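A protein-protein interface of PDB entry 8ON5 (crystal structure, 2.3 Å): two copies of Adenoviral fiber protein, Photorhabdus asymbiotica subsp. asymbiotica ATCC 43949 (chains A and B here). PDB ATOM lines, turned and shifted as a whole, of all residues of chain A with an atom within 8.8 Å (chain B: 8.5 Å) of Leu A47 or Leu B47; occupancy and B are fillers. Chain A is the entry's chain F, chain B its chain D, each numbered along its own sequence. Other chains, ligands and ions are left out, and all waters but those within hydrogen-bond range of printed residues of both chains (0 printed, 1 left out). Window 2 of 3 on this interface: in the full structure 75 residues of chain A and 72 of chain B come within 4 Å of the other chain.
CZ of Phe A44 touches CE1 of Phe B44 (3.7 Å). CD2 of Leu A47 touches CD2 of Leu B47 (3.7 Å). Leu A47 touches Ile B48 (CD1 to CG1, 3.9 Å). Leu A47 touches Ala B51 (CD1 to CB, 3.9 Å). Ala B51 touches Leu A50. Glu B52 touches Leu A50. CB of Ala A51 touches CB of Ala B51, 3.8 Å away.
Leu A40 touches none of the printed residues of chain B. Printed residues of chain B within 4 Å of Phe A44: Phe B44. Of chain B, only Leu B47 (3.7 Å), Ile B48 (3.9 Å) and Ala B51 (3.9 Å) come within 4 Å of Leu A47. Printed residues of chain B within 4 Å of Leu A50: Ala B51 (3.6 Å) and Glu B52 (3.6 Å). Asp B43 touches none of the printed residues of chain A. Of the printed residues of chain A, Phe B44 touches Phe A44. Of chain A, only Leu A47 comes within 4 Å of Leu B47. The nearest residue of chain B that does not touch Leu A47 is Phe B44 (5.1 Å).
Printed residues of chain A that touch a printed residue of chain B: Phe A44, Leu A47, Leu A50 and Ala A51. Of the 14 printed residues of chain B, 5 touch a printed residue of chain A. Hydrophobic or aromatic side chains of chain B within 4 Å of the printed part of chain A: Phe B44, Leu B47, Ile B48 and Ala B51.
Phe B44 touches its own counterpart, Phe A44. Leu B47 touches its own counterpart, Leu A47. Leu A50 touches Glu B52, but with the chains exchanged Glu A52 does not touch Leu B50 (8.4 Å). Ala B51 touches its own counterpart, Ala A51.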
ATOM      1  N   LEU A  40     -17.690 -23.719   7.078  1.00  0.00           N
ATOM      2  CA  LEU A  40     -16.998 -22.589   6.470  1.00  0.00           C
ATOM      3  C   LEU A  40     -17.115 -21.324   7.322  1.00  0.00           C
ATOM      4  O   LEU A  40     -16.169 -20.540   7.349  1.00  0.00           O
ATOM      5  CB  LEU A  40     -17.567 -22.304   5.089  1.00  0.00           C
ATOM      6  CG  LEU A  40     -16.841 -22.989   3.943  1.00  0.00           C
ATOM      7  CD1 LEU A  40     -17.580 -22.704   2.650  1.00  0.00           C
ATOM      8  CD2 LEU A  40     -15.393 -22.528   3.841  1.00  0.00           C
ATOM      9  N   GLU A  41     -18.268 -21.111   7.975  1.00  0.00           N
ATOM     10  CA  GLU A  41     -18.455 -19.943   8.829  1.00  0.00           C
ATOM     11  C   GLU A  41     -17.539 -20.023  10.044  1.00  0.00           C
ATOM     12  O   GLU A  41     -16.961 -19.015  10.443  1.00  0.00           O
ATOM     13  CB  GLU A  41     -19.898 -19.780   9.318  1.00  0.00           C
ATOM     14  CG  GLU A  41     -20.716 -18.881   8.427  1.00  0.00           C
ATOM     15  CD  GLU A  41     -22.137 -18.618   8.903  1.00  0.00           C
ATOM     16  OE1 GLU A  41     -22.593 -19.262   9.880  1.00  0.00           O
ATOM     17  OE2 GLU A  41     -22.779 -17.759   8.293  1.00  0.00           O
ATOM     18  N   THR A  42     -17.434 -21.222  10.628  1.00  0.00           N
ATOM     19  CA  THR A  42     -16.585 -21.429  11.780  1.00  0.00           C
ATOM     20  C   THR A  42     -15.160 -21.129  11.363  1.00  0.00           C
ATOM     21  O   THR A  42     -14.503 -20.327  12.011  1.00  0.00           O
ATOM     22  CB  THR A  42     -16.765 -22.824  12.368  1.00  0.00           C
ATOM     23  OG1 THR A  42     -18.177 -22.949  12.542  1.00  0.00           O
ATOM     24  CG2 THR A  42     -16.022 -23.001  13.676  1.00  0.00           C
ATOM     25  N   ASP A  43     -14.735 -21.682  10.226  1.00  0.00           N
ATOM     26  CA  ASP A  43     -13.368 -21.483   9.774  1.00  0.00           C
ATOM     27  C   ASP A  43     -13.067 -19.990   9.612  1.00  0.00           C
ATOM     28  O   ASP A  43     -12.016 -19.530  10.039  1.00  0.00           O
ATOM     29  CB  ASP A  43     -13.057 -22.307   8.521  1.00  0.00           C
ATOM     30  CG  ASP A  43     -12.866 -23.807   8.792  1.00  0.00           C
ATOM     31  OD1 ASP A  43     -12.896 -24.230   9.982  1.00  0.00           O
ATOM     32  OD2 ASP A  43     -12.697 -24.562   7.824  1.00  0.00           O
ATOM     33  N   PHE A  44     -13.975 -19.218   9.012  1.00  0.00           N
ATOM     34  CA  PHE A  44     -13.689 -17.822   8.717  1.00  0.00           C
ATOM     35  C   PHE A  44     -13.725 -16.989   9.996  1.00  0.00           C
ATOM     36  O   PHE A  44     -12.917 -16.091  10.145  1.00  0.00           O
ATOM     37  CB  PHE A  44     -14.605 -17.287   7.616  1.00  0.00           C
ATOM     38  CG  PHE A  44     -14.062 -17.558   6.241  1.00  0.00           C
ATOM     39  CD1 PHE A  44     -12.963 -16.864   5.776  1.00  0.00           C
ATOM     40  CD2 PHE A  44     -14.598 -18.552   5.439  1.00  0.00           C
ATOM     41  CE1 PHE A  44     -12.442 -17.119   4.516  1.00  0.00           C
ATOM     42  CE2 PHE A  44     -14.078 -18.801   4.178  1.00  0.00           C
ATOM     43  CZ  PHE A  44     -12.996 -18.096   3.719  1.00  0.00           C
ATOM     44  N   THR A  45     -14.591 -17.374  10.931  1.00  0.00           N
ATOM     45  CA  THR A  45     -14.690 -16.789  12.251  1.00  0.00           C
ATOM     46  C   THR A  45     -13.363 -16.935  12.997  1.00  0.00           C
ATOM     47  O   THR A  45     -12.853 -15.975  13.576  1.00  0.00           O
ATOM     48  CB  THR A  45     -15.907 -17.410  12.958  1.00  0.00           C
ATOM     49  OG1 THR A  45     -16.999 -16.739  12.333  1.00  0.00           O
ATOM     50  CG2 THR A  45     -15.965 -17.221  14.463  1.00  0.00           C
ATOM     51  N   ASN A  46     -12.821 -18.154  12.987  1.00  0.00           N
ATOM     52  CA  ASN A  46     -11.592 -18.456  13.681  1.00  0.00           C
ATOM     53  C   ASN A  46     -10.406 -17.807  12.974  1.00  0.00           C
ATOM     54  O   ASN A  46      -9.427 -17.434  13.621  1.00  0.00           O
ATOM     55  CB  ASN A  46     -11.397 -19.969  13.849  1.00  0.00           C
ATOM     56  CG  ASN A  46     -12.333 -20.564  14.882  1.00  0.00           C
ATOM     57  OD1 ASN A  46     -12.752 -21.714  14.787  1.00  0.00           O
ATOM     58  ND2 ASN A  46     -12.634 -19.798  15.908  1.00  0.00           N
ATOM     59  N   LEU A  47     -10.448 -17.693  11.652  1.00  0.00           N
ATOM     60  CA  LEU A  47      -9.303 -17.102  10.983  1.00  0.00           C
ATOM     61  C   LEU A  47      -9.279 -15.597  11.243  1.00  0.00           C
ATOM     62  O   LEU A  47      -8.216 -14.996  11.298  1.00  0.00           O
ATOM     63  CB  LEU A  47      -9.365 -17.408   9.488  1.00  0.00           C
ATOM     64  CG  LEU A  47      -8.375 -16.666   8.602  1.00  0.00           C
ATOM     65  CD1 LEU A  47      -6.937 -16.975   9.011  1.00  0.00           C
ATOM     66  CD2 LEU A  47      -8.606 -17.011   7.141  1.00  0.00           C
ATOM     67  N   ILE A  48     -10.455 -14.971  11.372  1.00  0.00           N
ATOM     68  CA  ILE A  48     -10.494 -13.531  11.563  1.00  0.00           C
ATOM     69  C   ILE A  48      -9.982 -13.180  12.965  1.00  0.00           C
ATOM     70  O   ILE A  48      -9.192 -12.247  13.125  1.00  0.00           O
ATOM     71  CB  ILE A  48     -11.903 -12.979  11.272  1.00  0.00           C
ATOM     72  CG1 ILE A  48     -12.133 -12.860   9.767  1.00  0.00           C
ATOM     73  CG2 ILE A  48     -12.144 -11.652  11.983  1.00  0.00           C
ATOM     74  CD1 ILE A  48     -13.589 -12.871   9.361  1.00  0.00           C
ATOM     75  N   ASP A  49     -10.434 -13.937  13.967  1.00  0.00           N
ATOM     76  CA  ASP A  49     -10.009 -13.755  15.339  1.00  0.00           C
ATOM     77  C   ASP A  49      -8.508 -14.046  15.497  1.00  0.00           C
ATOM     78  O   ASP A  49      -7.836 -13.405  16.316  1.00  0.00           O
ATOM     79  CB  ASP A  49     -10.857 -14.636  16.256  1.00  0.00           C
ATOM     80  CG  ASP A  49     -12.260 -14.101  16.467  1.00  0.00           C
ATOM     81  OD1 ASP A  49     -12.502 -12.907  16.137  1.00  0.00           O
ATOM     82  OD2 ASP A  49     -13.102 -14.875  16.953  1.00  0.00           O
ATOM     83  N   LEU A  50      -7.980 -15.019  14.727  1.00  0.00           N
ATOM     84  CA  LEU A  50      -6.555 -15.317  14.758  1.00  0.00           C
ATOM     85  C   LEU A  50      -5.804 -14.091  14.269  1.00  0.00           C
ATOM     86  O   LEU A  50      -4.863 -13.649  14.911  1.00  0.00           O
ATOM     87  CB  LEU A  50      -6.236 -16.534  13.879  1.00  0.00           C
ATOM     88  CG  LEU A  50      -4.786 -17.009  13.827  1.00  0.00           C
ATOM     89  CD1 LEU A  50      -4.208 -17.184  15.224  1.00  0.00           C
ATOM     90  CD2 LEU A  50      -4.694 -18.340  13.083  1.00  0.00           C
ATOM     91  N   ALA A  51      -6.214 -13.544  13.132  1.00  0.00           N
ATOM     92  CA  ALA A  51      -5.482 -12.424  12.553  1.00  0.00           C
ATOM     93  C   ALA A  51      -5.644 -11.145  13.390  1.00  0.00           C
ATOM     94  O   ALA A  51      -4.874 -10.201  13.230  1.00  0.00           O
ATOM     95  CB  ALA A  51      -5.941 -12.209  11.138  1.00  0.00           C
ATOM     96  N   GLU A  52      -6.655 -11.123  14.269  1.00  0.00           N
ATOM     97  CA  GLU A  52      -6.940  -9.999  15.141  1.00  0.00           C
ATOM     98  C   GLU A  52      -5.902  -9.917  16.273  1.00  0.00           C
ATOM     99  O   GLU A  52      -5.661  -8.845  16.842  1.00  0.00           O
ATOM    100  CB  GLU A  52      -8.380 -10.149  15.629  1.00  0.00           C
ATOM    101  CG  GLU A  52      -8.794  -9.234  16.770  1.00  0.00           C
ATOM    102  CD  GLU A  52      -8.960  -7.755  16.442  1.00  0.00           C
ATOM    103  OE1 GLU A  52      -9.488  -7.047  17.322  1.00  0.00           O
ATOM    104  OE2 GLU A  52      -8.541  -7.306  15.337  1.00  0.00           O
ATOM    105  N   VAL A  53      -5.274 -11.051  16.602  1.00  0.00           N
ATOM    106  CA  VAL A  53      -4.409 -11.130  17.763  1.00  0.00           C
ATOM    107  C   VAL A  53      -3.287 -10.100  17.634  1.00  0.00           C
ATOM    108  O   VAL A  53      -2.900  -9.495  18.632  1.00  0.00           O
ATOM    109  CB  VAL A  53      -3.833 -12.548  17.948  1.00  0.00           C
ATOM    110  CG1 VAL A  53      -2.748 -12.566  19.019  1.00  0.00           C
ATOM    111  CG2 VAL A  53      -4.927 -13.561  18.265  1.00  0.00           C
ATOM    112  N   LEU B  40      -5.752 -22.235  -4.764  1.00  0.00           N
ATOM    113  CA  LEU B  40      -6.539 -21.838  -3.601  1.00  0.00           C
ATOM    114  C   LEU B  40      -5.921 -22.396  -2.330  1.00  0.00           C
ATOM    115  O   LEU B  40      -5.857 -21.684  -1.335  1.00  0.00           O
ATOM    116  CB  LEU B  40      -7.991 -22.328  -3.689  1.00  0.00           C
ATOM    117  CG  LEU B  40      -9.018 -21.383  -4.305  1.00  0.00           C
ATOM    118  CD1 LEU B  40     -10.398 -22.004  -4.222  1.00  0.00           C
ATOM    119  CD2 LEU B  40      -9.035 -20.042  -3.611  1.00  0.00           C
ATOM    120  N   GLU B  41      -5.549 -23.682  -2.329  1.00  0.00           N
ATOM    121  CA  GLU B  41      -5.028 -24.294  -1.112  1.00  0.00           C
ATOM    122  C   GLU B  41      -3.770 -23.560  -0.636  1.00  0.00           C
ATOM    123  O   GLU B  41      -3.531 -23.453   0.557  1.00  0.00           O
ATOM    124  CB  GLU B  41      -4.712 -25.775  -1.302  1.00  0.00           C
ATOM    125  CG  GLU B  41      -5.879 -26.664  -0.957  1.00  0.00           C
ATOM    126  CD  GLU B  41      -5.555 -28.146  -0.871  1.00  0.00           C
ATOM    127  OE1 GLU B  41      -6.408 -28.894  -0.354  1.00  0.00           O
ATOM    128  OE2 GLU B  41      -4.457 -28.546  -1.320  1.00  0.00           O
ATOM    129  N   THR B  42      -2.971 -23.090  -1.594  1.00  0.00           N
ATOM    130  CA  THR B  42      -1.709 -22.446  -1.334  1.00  0.00           C
ATOM    131  C   THR B  42      -1.985 -21.055  -0.750  1.00  0.00           C
ATOM    132  O   THR B  42      -1.304 -20.627   0.179  1.00  0.00           O
ATOM    133  CB  THR B  42      -0.866 -22.530  -2.616  1.00  0.00           C
ATOM    134  OG1 THR B  42      -0.536 -23.917  -2.710  1.00  0.00           O
ATOM    135  CG2 THR B  42       0.386 -21.677  -2.627  1.00  0.00           C
ATOM    136  N   ASP B  43      -3.014 -20.366  -1.247  1.00  0.00           N
ATOM    137  CA  ASP B  43      -3.330 -19.039  -0.754  1.00  0.00           C
ATOM    138  C   ASP B  43      -3.890 -19.085   0.675  1.00  0.00           C
ATOM    139  O   ASP B  43      -3.459 -18.292   1.515  1.00  0.00           O
ATOM    140  CB  ASP B  43      -4.248 -18.304  -1.730  1.00  0.00           C
ATOM    141  CG  ASP B  43      -3.571 -18.024  -3.060  1.00  0.00           C
ATOM    142  OD1 ASP B  43      -2.364 -18.330  -3.187  1.00  0.00           O
ATOM    143  OD2 ASP B  43      -4.258 -17.525  -3.969  1.00  0.00           O
ATOM    144  N   PHE B  44      -4.840 -19.990   0.952  1.00  0.00           N
ATOM    145  CA  PHE B  44      -5.399 -20.129   2.290  1.00  0.00           C
ATOM    146  C   PHE B  44      -4.340 -20.573   3.304  1.00  0.00           C
ATOM    147  O   PHE B  44      -4.423 -20.183   4.462  1.00  0.00           O
ATOM    148  CB  PHE B  44      -6.630 -21.044   2.291  1.00  0.00           C
ATOM    149  CG  PHE B  44      -7.891 -20.339   1.860  1.00  0.00           C
ATOM    150  CD1 PHE B  44      -8.542 -19.468   2.721  1.00  0.00           C
ATOM    151  CD2 PHE B  44      -8.391 -20.482   0.579  1.00  0.00           C
ATOM    152  CE1 PHE B  44      -9.681 -18.784   2.320  1.00  0.00           C
ATOM    153  CE2 PHE B  44      -9.527 -19.795   0.175  1.00  0.00           C
ATOM    154  CZ  PHE B  44     -10.176 -18.949   1.047  1.00  0.00           C
ATOM    155  N   THR B  45      -3.381 -21.407   2.882  1.00  0.00           N
ATOM    156  CA  THR B  45      -2.293 -21.855   3.736  1.00  0.00           C
ATOM    157  C   THR B  45      -1.438 -20.653   4.177  1.00  0.00           C
ATOM    158  O   THR B  45      -1.177 -20.452   5.359  1.00  0.00           O
ATOM    159  CB  THR B  45      -1.518 -22.982   3.023  1.00  0.00           C
ATOM    160  OG1 THR B  45      -2.358 -24.128   3.155  1.00  0.00           O
ATOM    161  CG2 THR B  45      -0.164 -23.302   3.622  1.00  0.00           C
ATOM    162  N   ASN B  46      -1.020 -19.865   3.199  1.00  0.00           N
ATOM    163  CA  ASN B  46      -0.231 -18.675   3.389  1.00  0.00           C
ATOM    164  C   ASN B  46      -0.973 -17.668   4.273  1.00  0.00           C
ATOM    165  O   ASN B  46      -0.384 -17.098   5.184  1.00  0.00           O
ATOM    166  CB  ASN B  46       0.189 -18.125   2.021  1.00  0.00           C
ATOM    167  CG  ASN B  46       1.275 -18.969   1.384  1.00  0.00           C
ATOM    168  OD1 ASN B  46       1.839 -19.851   2.029  1.00  0.00           O
ATOM    169  ND2 ASN B  46       1.571 -18.724   0.121  1.00  0.00           N
ATOM    170  N   LEU B  47      -2.263 -17.471   4.023  1.00  0.00           N
ATOM    171  CA  LEU B  47      -3.021 -16.496   4.772  1.00  0.00           C
ATOM    172  C   LEU B  47      -3.133 -16.922   6.229  1.00  0.00           C
ATOM    173  O   LEU B  47      -3.073 -16.070   7.107  1.00  0.00           O
ATOM    174  CB  LEU B  47      -4.394 -16.273   4.136  1.00  0.00           C
ATOM    175  CG  LEU B  47      -5.372 -15.453   4.979  1.00  0.00           C
ATOM    176  CD1 LEU B  47      -4.851 -14.034   5.175  1.00  0.00           C
ATOM    177  CD2 LEU B  47      -6.767 -15.414   4.358  1.00  0.00           C
ATOM    178  N   ILE B  48      -3.319 -18.217   6.479  1.00  0.00           N
ATOM    179  CA  ILE B  48      -3.464 -18.732   7.832  1.00  0.00           C
ATOM    180  C   ILE B  48      -2.132 -18.607   8.575  1.00  0.00           C
ATOM    181  O   ILE B  48      -2.110 -18.338   9.765  1.00  0.00           O
ATOM    182  CB  ILE B  48      -3.985 -20.178   7.796  1.00  0.00           C
ATOM    183  CG1 ILE B  48      -5.455 -20.214   7.377  1.00  0.00           C
ATOM    184  CG2 ILE B  48      -3.777 -20.891   9.118  1.00  0.00           C
ATOM    185  CD1 ILE B  48      -5.929 -21.584   6.957  1.00  0.00           C
ATOM    186  N   ASP B  49      -1.028 -18.833   7.870  1.00  0.00           N
ATOM    187  CA  ASP B  49       0.289 -18.725   8.466  1.00  0.00           C
ATOM    188  C   ASP B  49       0.645 -17.254   8.693  1.00  0.00           C
ATOM    189  O   ASP B  49       1.354 -16.958   9.633  1.00  0.00           O
ATOM    190  CB  ASP B  49       1.345 -19.451   7.630  1.00  0.00           C
ATOM    191  CG  ASP B  49       1.320 -20.970   7.792  1.00  0.00           C
ATOM    192  OD1 ASP B  49       0.611 -21.473   8.707  1.00  0.00           O
ATOM    193  OD2 ASP B  49       1.961 -21.657   6.952  1.00  0.00           O
ATOM    194  N   LEU B  50       0.187 -16.347   7.829  1.00  0.00           N
ATOM    195  CA  LEU B  50       0.308 -14.927   8.085  1.00  0.00           C
ATOM    196  C   LEU B  50      -0.413 -14.548   9.375  1.00  0.00           C
ATOM    197  O   LEU B  50       0.184 -13.917  10.233  1.00  0.00           O
ATOM    198  CB  LEU B  50      -0.251 -14.153   6.899  1.00  0.00           C
ATOM    199  CG  LEU B  50      -0.047 -12.647   6.979  1.00  0.00           C
ATOM    200  CD1 LEU B  50       1.428 -12.314   7.157  1.00  0.00           C
ATOM    201  CD2 LEU B  50      -0.580 -11.973   5.730  1.00  0.00           C
ATOM    202  N   ALA B  51      -1.673 -14.973   9.531  1.00  0.00           N
ATOM    203  CA  ALA B  51      -2.464 -14.727  10.735  1.00  0.00           C
ATOM    204  C   ALA B  51      -1.803 -15.243  12.015  1.00  0.00           C
ATOM    205  O   ALA B  51      -1.888 -14.581  13.046  1.00  0.00           O
ATOM    206  CB  ALA B  51      -3.827 -15.347  10.606  1.00  0.00           C
ATOM    207  N   GLU B  52      -1.172 -16.417  11.944  1.00  0.00           N
ATOM    208  CA  GLU B  52      -0.610 -17.122  13.088  1.00  0.00           C
ATOM    209  C   GLU B  52       0.558 -16.345  13.744  1.00  0.00           C
ATOM    210  O   GLU B  52       0.808 -16.483  14.943  1.00  0.00           O
ATOM    211  CB  GLU B  52      -0.181 -18.507  12.580  1.00  0.00           C
ATOM    212  CG  GLU B  52       0.576 -19.360  13.596  1.00  0.00           C
ATOM    213  CD  GLU B  52      -0.133 -19.758  14.878  1.00  0.00           C
ATOM    214  OE1 GLU B  52       0.404 -20.648  15.563  1.00  0.00           O
ATOM    215  OE2 GLU B  52      -1.228 -19.225  15.188  1.00  0.00           O
ATOM    216  N   VAL B  53       1.277 -15.524  12.958  1.00  0.00           N
ATOM    217  CA  VAL B  53       2.463 -14.798  13.390  1.00  0.00           C
ATOM    218  C   VAL B  53       2.186 -13.997  14.661  1.00  0.00           C
ATOM    219  O   VAL B  53       2.982 -13.994  15.601  1.00  0.00           O
ATOM    220  CB  VAL B  53       2.944 -13.849  12.280  1.00  0.00           C
ATOM    221  CG1 VAL B  53       3.984 -12.868  12.818  1.00  0.00           C
ATOM    222  CG2 VAL B  53       3.448 -14.607  11.047  1.00  0.00           C
